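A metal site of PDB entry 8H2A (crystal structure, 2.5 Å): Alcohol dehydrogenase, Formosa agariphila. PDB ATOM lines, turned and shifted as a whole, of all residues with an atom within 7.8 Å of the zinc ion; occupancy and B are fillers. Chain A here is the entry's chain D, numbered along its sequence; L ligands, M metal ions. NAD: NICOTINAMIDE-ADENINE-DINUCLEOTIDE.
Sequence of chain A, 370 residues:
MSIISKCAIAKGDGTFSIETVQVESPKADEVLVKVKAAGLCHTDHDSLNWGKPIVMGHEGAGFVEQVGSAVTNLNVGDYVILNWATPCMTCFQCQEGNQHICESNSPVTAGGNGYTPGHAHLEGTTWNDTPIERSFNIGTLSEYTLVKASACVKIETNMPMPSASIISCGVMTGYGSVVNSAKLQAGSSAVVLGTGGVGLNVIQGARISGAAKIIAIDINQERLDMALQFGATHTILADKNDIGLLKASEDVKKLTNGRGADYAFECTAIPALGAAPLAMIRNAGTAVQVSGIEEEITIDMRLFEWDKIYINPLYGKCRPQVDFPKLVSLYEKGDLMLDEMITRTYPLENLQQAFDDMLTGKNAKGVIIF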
ATOM      1  N   GLY A  39      12.271 -32.230 -31.133  1.00  0.00           N
ATOM      2  CA  GLY A  39      13.103 -31.289 -30.414  1.00  0.00           C
ATOM      3  C   GLY A  39      12.550 -31.004 -29.023  1.00  0.00           C
ATOM      4  O   GLY A  39      11.396 -31.307 -28.731  1.00  0.00           O
ATOM      5  N   LEU A  40      13.396 -30.403 -28.174  1.00  0.00           N
ATOM      6  CA  LEU A  40      13.075 -30.218 -26.762  1.00  0.00           C
ATOM      7  C   LEU A  40      13.341 -28.771 -26.365  1.00  0.00           C
ATOM      8  O   LEU A  40      14.084 -28.060 -27.021  1.00  0.00           O
ATOM      9  CB  LEU A  40      13.890 -31.171 -25.875  1.00  0.00           C
ATOM     10  CG  LEU A  40      13.403 -31.504 -24.458  1.00  0.00           C
ATOM     11  CD1 LEU A  40      12.228 -32.458 -24.492  1.00  0.00           C
ATOM     12  CD2 LEU A  40      14.539 -32.072 -23.612  1.00  0.00           C
ATOM     13  N   CYS A  41      12.708 -28.359 -25.259  1.00  0.00           N
ATOM     14  CA  CYS A  41      12.805 -26.990 -24.760  1.00  0.00           C
ATOM     15  C   CYS A  41      12.487 -26.985 -23.275  1.00  0.00           C
ATOM     16  O   CYS A  41      12.053 -27.982 -22.713  1.00  0.00           O
ATOM     17  CB  CYS A  41      11.862 -26.042 -25.502  1.00  0.00           C
ATOM     18  SG  CYS A  41      12.458 -25.476 -27.107  1.00  0.00           S
ATOM     19  N   HIS A  42      12.647 -25.828 -22.648  1.00  0.00           N
ATOM     20  CA  HIS A  42      12.308 -25.724 -21.235  1.00  0.00           C
ATOM     21  C   HIS A  42      10.804 -25.765 -20.975  1.00  0.00           C
ATOM     22  O   HIS A  42      10.411 -26.113 -19.868  1.00  0.00           O
ATOM     23  CB  HIS A  42      13.035 -24.522 -20.614  1.00  0.00           C
ATOM     24  CG  HIS A  42      12.574 -24.177 -19.230  1.00  0.00           C
ATOM     25  ND1 HIS A  42      12.594 -25.101 -18.193  1.00  0.00           N
ATOM     26  CD2 HIS A  42      12.338 -22.966 -18.653  1.00  0.00           C
ATOM     27  CE1 HIS A  42      12.207 -24.497 -17.077  1.00  0.00           C
ATOM     28  NE2 HIS A  42      12.077 -23.197 -17.324  1.00  0.00           N
ATOM     29  N   THR A  43       9.982 -25.499 -21.985  1.00  0.00           N
ATOM     30  CA  THR A  43       8.539 -25.647 -21.830  1.00  0.00           C
ATOM     31  C   THR A  43       8.134 -27.098 -21.597  1.00  0.00           C
ATOM     32  O   THR A  43       7.151 -27.359 -20.898  1.00  0.00           O
ATOM     33  CB  THR A  43       7.830 -25.064 -23.059  1.00  0.00           C
ATOM     34  OG1 THR A  43       8.176 -23.673 -23.166  1.00  0.00           O
ATOM     35  CG2 THR A  43       6.304 -25.200 -22.947  1.00  0.00           C
ATOM     36  N   ASP A  44       8.865 -28.045 -22.193  1.00  0.00           N
ATOM     37  CA  ASP A  44       8.642 -29.457 -21.908  1.00  0.00           C
ATOM     38  C   ASP A  44       8.980 -29.808 -20.467  1.00  0.00           C
ATOM     39  O   ASP A  44       8.309 -30.634 -19.840  1.00  0.00           O
ATOM     40  CB  ASP A  44       9.455 -30.316 -22.887  1.00  0.00           C
ATOM     41  CG  ASP A  44       8.785 -30.473 -24.226  1.00  0.00           C
ATOM     42  OD1 ASP A  44       7.550 -30.654 -24.268  1.00  0.00           O
ATOM     43  OD2 ASP A  44       9.488 -30.393 -25.251  1.00  0.00           O
ATOM     44  N   HIS A  58       6.335 -30.673 -27.970  1.00  0.00           N
ATOM     45  CA  HIS A  58       5.656 -29.684 -28.799  1.00  0.00           C
ATOM     46  C   HIS A  58       6.423 -29.380 -30.070  1.00  0.00           C
ATOM     47  O   HIS A  58       6.020 -28.473 -30.814  1.00  0.00           O
ATOM     48  CB  HIS A  58       5.405 -28.388 -28.016  1.00  0.00           C
ATOM     49  CG  HIS A  58       6.648 -27.751 -27.455  1.00  0.00           C
ATOM     50  ND1 HIS A  58       7.250 -28.194 -26.290  1.00  0.00           N
ATOM     51  CD2 HIS A  58       7.386 -26.711 -27.892  1.00  0.00           C
ATOM     52  CE1 HIS A  58       8.316 -27.450 -26.044  1.00  0.00           C
ATOM     53  NE2 HIS A  58       8.421 -26.544 -26.997  1.00  0.00           N
ATOM     54  N   GLU A  59       7.517 -30.089 -30.333  1.00  0.00           N
ATOM     55  CA  GLU A  59       8.344 -29.924 -31.521  1.00  0.00           C
ATOM     56  C   GLU A  59       8.434 -31.258 -32.232  1.00  0.00           C
ATOM     57  O   GLU A  59       8.778 -32.271 -31.614  1.00  0.00           O
ATOM     58  CB  GLU A  59       9.743 -29.403 -31.143  1.00  0.00           C
ATOM     59  CG  GLU A  59       9.672 -28.048 -30.463  1.00  0.00           C
ATOM     60  CD  GLU A  59      10.929 -27.666 -29.680  1.00  0.00           C
ATOM     61  OE1 GLU A  59      10.850 -27.599 -28.440  1.00  0.00           O
ATOM     62  OE2 GLU A  59      11.981 -27.393 -30.306  1.00  0.00           O
ATOM     63  N   TRP A  84       2.149 -26.129 -33.241  1.00  0.00           N
ATOM     64  CA  TRP A  84       1.310 -26.127 -32.046  1.00  0.00           C
ATOM     65  C   TRP A  84       0.296 -24.982 -32.058  1.00  0.00           C
ATOM     66  O   TRP A  84      -0.402 -24.779 -31.057  1.00  0.00           O
ATOM     67  CB  TRP A  84       2.168 -26.103 -30.769  1.00  0.00           C
ATOM     68  CG  TRP A  84       3.254 -25.081 -30.711  1.00  0.00           C
ATOM     69  CD1 TRP A  84       4.522 -25.218 -31.193  1.00  0.00           C
ATOM     70  CD2 TRP A  84       3.194 -23.786 -30.091  1.00  0.00           C
ATOM     71  NE1 TRP A  84       5.253 -24.082 -30.919  1.00  0.00           N
ATOM     72  CE2 TRP A  84       4.462 -23.183 -30.252  1.00  0.00           C
ATOM     73  CE3 TRP A  84       2.189 -23.074 -29.432  1.00  0.00           C
ATOM     74  CZ2 TRP A  84       4.755 -21.899 -29.782  1.00  0.00           C
ATOM     75  CZ3 TRP A  84       2.482 -21.790 -28.962  1.00  0.00           C
ATOM     76  CH2 TRP A  84       3.756 -21.217 -29.153  1.00  0.00           C
ATOM     77  N   SER A 165      12.628 -30.432 -36.973  1.00  0.00           N
ATOM     78  CA  SER A 165      11.843 -30.417 -35.734  1.00  0.00           C
ATOM     79  C   SER A 165      12.016 -29.115 -34.978  1.00  0.00           C
ATOM     80  O   SER A 165      11.122 -28.730 -34.222  1.00  0.00           O
ATOM     81  CB  SER A 165      12.183 -31.611 -34.824  1.00  0.00           C
ATOM     82  OG  SER A 165      13.434 -31.476 -34.178  1.00  0.00           O
ATOM     83  N   ILE A 166      13.145 -28.410 -35.162  1.00  0.00           N
ATOM     84  CA  ILE A 166      13.341 -27.166 -34.421  1.00  0.00           C
ATOM     85  C   ILE A 166      12.627 -25.987 -35.053  1.00  0.00           C
ATOM     86  O   ILE A 166      12.525 -24.939 -34.412  1.00  0.00           O
ATOM     87  CB  ILE A 166      14.828 -26.841 -34.228  1.00  0.00           C
ATOM     88  CG1 ILE A 166      15.548 -26.770 -35.576  1.00  0.00           C
ATOM     89  CG2 ILE A 166      15.445 -27.879 -33.364  1.00  0.00           C
ATOM     90  CD1 ILE A 166      16.967 -26.311 -35.466  1.00  0.00           C
ATOM     91  N   SER A 168       9.550 -26.186 -35.476  1.00  0.00           N
ATOM     92  CA  SER A 168       8.286 -26.265 -34.759  1.00  0.00           C
ATOM     93  C   SER A 168       8.192 -25.296 -33.587  1.00  0.00           C
ATOM     94  O   SER A 168       7.083 -25.086 -33.060  1.00  0.00           O
ATOM     95  CB  SER A 168       8.095 -27.708 -34.299  1.00  0.00           C
ATOM     96  OG  SER A 168       6.994 -27.818 -33.414  1.00  0.00           O
ATOM     97  N   CYS A 169       9.299 -24.689 -33.165  1.00  0.00           N
ATOM     98  CA  CYS A 169       9.279 -23.850 -31.982  1.00  0.00           C
ATOM     99  C   CYS A 169      10.348 -22.777 -32.023  1.00  0.00           C
ATOM    100  O   CYS A 169      10.072 -21.639 -32.425  1.00  0.00           O
ATOM    101  CB  CYS A 169       9.475 -24.687 -30.722  1.00  0.00           C
ATOM    102  SG  CYS A 169       9.255 -23.806 -29.148  1.00  0.00           S
ATOM    103  N   GLY A 170      11.581 -23.125 -31.630  1.00  0.00           N
ATOM    104  CA  GLY A 170      12.616 -22.125 -31.491  1.00  0.00           C
ATOM    105  C   GLY A 170      12.853 -21.312 -32.749  1.00  0.00           C
ATOM    106  O   GLY A 170      13.100 -20.115 -32.676  1.00  0.00           O
ATOM    107  N   VAL A 171      12.764 -21.940 -33.910  1.00  0.00           N
ATOM    108  CA  VAL A 171      13.082 -21.213 -35.138  1.00  0.00           C
ATOM    109  C   VAL A 171      11.916 -20.306 -35.558  1.00  0.00           C
ATOM    110  O   VAL A 171      12.131 -19.151 -35.949  1.00  0.00           O
ATOM    111  CB  VAL A 171      13.486 -22.195 -36.253  1.00  0.00           C
ATOM    112  CG1 VAL A 171      13.889 -21.453 -37.508  1.00  0.00           C
ATOM    113  CG2 VAL A 171      14.632 -23.098 -35.763  1.00  0.00           C
ATOM    114  N   THR A 173       9.502 -19.015 -33.629  1.00  0.00           N
ATOM    115  CA  THR A 173       9.287 -17.889 -32.721  1.00  0.00           C
ATOM    116  C   THR A 173      10.422 -16.870 -32.841  1.00  0.00           C
ATOM    117  O   THR A 173      10.170 -15.659 -32.772  1.00  0.00           O
ATOM    118  CB  THR A 173       9.125 -18.368 -31.261  1.00  0.00           C
ATOM    119  OG1 THR A 173      10.402 -18.653 -30.698  1.00  0.00           O
ATOM    120  CG2 THR A 173       8.283 -19.625 -31.205  1.00  0.00           C
ATOM    121  N   VAL A 198      15.787 -19.762 -28.603  1.00  0.00           N
ATOM    122  CA  VAL A 198      15.033 -18.690 -29.251  1.00  0.00           C
ATOM    123  C   VAL A 198      15.993 -17.704 -29.902  1.00  0.00           C
ATOM    124  O   VAL A 198      15.980 -17.517 -31.129  1.00  0.00           O
ATOM    125  CB  VAL A 198      14.100 -17.991 -28.245  1.00  0.00           C
ATOM    126  CG1 VAL A 198      13.412 -16.802 -28.906  1.00  0.00           C
ATOM    127  CG2 VAL A 198      13.064 -18.969 -27.737  1.00  0.00           C
ATOM    128  N   LYS A 365      19.974 -27.062 -27.962  1.00  0.00           N
ATOM    129  CA  LYS A 365      18.753 -27.749 -28.367  1.00  0.00           C
ATOM    130  C   LYS A 365      18.993 -29.245 -28.326  1.00  0.00           C
ATOM    131  O   LYS A 365      20.093 -29.710 -28.633  1.00  0.00           O
ATOM    132  CB  LYS A 365      18.297 -27.306 -29.783  1.00  0.00           C
ATOM    133  CG  LYS A 365      16.915 -27.781 -30.192  1.00  0.00           C
ATOM    134  CD  LYS A 365      15.808 -27.081 -29.414  1.00  0.00           C
ATOM    135  CE  LYS A 365      15.603 -25.632 -29.841  1.00  0.00           C
ATOM    136  NZ  LYS A 365      14.958 -25.496 -31.182  1.00  0.00           N
HETATM  137  PA  NAD L   1      17.678 -20.839 -23.456  1.00  0.00           P
HETATM  138  O1A NAD L   1      18.110 -21.324 -22.075  1.00  0.00           O
HETATM  139  O2A NAD L   1      18.448 -21.507 -24.630  1.00  0.00           O
HETATM  140  O5B NAD L   1      17.847 -19.157 -23.592  1.00  0.00           O
HETATM  141  C5B NAD L   1      18.165 -18.351 -22.469  1.00  0.00           C
HETATM  142  C4B NAD L   1      19.445 -17.554 -22.858  1.00  0.00           C
HETATM  143  O4B NAD L   1      19.443 -16.419 -22.201  1.00  0.00           O
HETATM  144  C3B NAD L   1      20.666 -18.389 -22.364  1.00  0.00           C
HETATM  145  O3B NAD L   1      21.658 -18.487 -23.312  1.00  0.00           O
HETATM  146  C2B NAD L   1      21.098 -17.617 -21.126  1.00  0.00           C
HETATM  147  O2B NAD L   1      22.511 -17.923 -20.832  1.00  0.00           O
HETATM  148  C1B NAD L   1      20.876 -16.355 -21.485  1.00  0.00           C
HETATM  149  N9A NAD L   1      20.868 -15.466 -20.342  1.00  0.00           N
HETATM  150  C8A NAD L   1      20.588 -15.785 -19.075  1.00  0.00           C
HETATM  151  N7A NAD L   1      20.727 -14.694 -18.342  1.00  0.00           N
HETATM  152  C5A NAD L   1      21.087 -13.684 -19.142  1.00  0.00           C
HETATM  153  C6A NAD L   1      21.350 -12.379 -18.888  1.00  0.00           C
HETATM  154  N6A NAD L   1      21.314 -11.698 -17.673  1.00  0.00           N
HETATM  155  N1A NAD L   1      21.699 -11.559 -19.866  1.00  0.00           N
HETATM  156  C2A NAD L   1      21.797 -12.028 -21.130  1.00  0.00           C
HETATM  157  N3A NAD L   1      21.551 -13.322 -21.385  1.00  0.00           N
HETATM  158  C4A NAD L   1      21.191 -14.161 -20.389  1.00  0.00           C
HETATM  159  O3  NAD L   1      16.096 -21.276 -23.667  1.00  0.00           O
HETATM  160  PN  NAD L   1      15.158 -20.458 -24.801  1.00  0.00           P
HETATM  161  O1N NAD L   1      14.404 -21.495 -25.625  1.00  0.00           O
HETATM  162  O2N NAD L   1      16.058 -19.618 -25.743  1.00  0.00           O
HETATM  163  O5D NAD L   1      14.223 -19.493 -23.909  1.00  0.00           O
HETATM  164  C5D NAD L   1      13.848 -18.236 -24.436  1.00  0.00           C
HETATM  165  C4D NAD L   1      12.461 -17.743 -23.913  1.00  0.00           C
HETATM  166  O4D NAD L   1      11.614 -17.564 -24.899  1.00  0.00           O
HETATM  167  C3D NAD L   1      11.825 -18.783 -22.920  1.00  0.00           C
HETATM  168  O3D NAD L   1      11.242 -18.089 -21.892  1.00  0.00           O
HETATM  169  C2D NAD L   1      10.759 -19.465 -23.744  1.00  0.00           C
HETATM  170  O2D NAD L   1       9.703 -19.958 -22.848  1.00  0.00           O
HETATM  171  C1D NAD L   1      10.318 -18.447 -24.499  1.00  0.00           C
HETATM  172  N1N NAD L   1       9.607 -18.908 -25.667  1.00  0.00           N
HETATM  173  C2N NAD L   1       8.554 -18.196 -26.090  1.00  0.00           C
HETATM  174  C3N NAD L   1       7.794 -18.614 -27.227  1.00  0.00           C
HETATM  175  C7N NAD L   1       6.627 -17.741 -27.640  1.00  0.00           C
HETATM  176  O7N NAD L   1       5.748 -18.184 -28.358  1.00  0.00           O
HETATM  177  N7N NAD L   1       6.596 -16.355 -27.117  1.00  0.00           N
HETATM  178  C4N NAD L   1       8.110 -19.734 -27.862  1.00  0.00           C
HETATM  179  C5N NAD L   1       9.165 -20.467 -27.427  1.00  0.00           C
HETATM  180  C6N NAD L   1       9.927 -20.033 -26.294  1.00  0.00           C
HETATM  181 ZN    ZN M   1      10.203 -25.274 -27.587  1.00  0.00          ZN
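An oxygen (O2N) of the ligand sits at hydrogen-bond distance from the backbone NH (N) of Val 198 (2.9 Å).
ND1 of His 58 lies within hydrogen-bond range of OD1 of Asp 44. O of His 58 sits at hydrogen-bond distance from OG of Ser 168, at 2.9 Å. OG1 of Thr 173 sits close to O of Cys 169 (3.5 Å). The side-chain carboxylate (OE2) of Glu 59 is in salt-bridge range of the side-chain amino group (NZ) of Lys 365, at 3.6 Å.
Within 4 Å of the zinc ion: Cys 41, His 58, Glu 59 and Cys 169. Along chain A the residues within 4 Å of the zinc ion span positions 41 to 169. The nearest printed residue that does not touch the zinc ion is Gly 170 (4.8 Å).
The zinc ion is bound by a ring nitrogen (NE2) of His 58, the side-chain sulfur (SG) of Cys 41, the side-chain sulfur (SG) of Cys 169 and the side-chain carboxylate (OE1) of Glu 59. The zinc ion has four donor atoms within binding distance.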
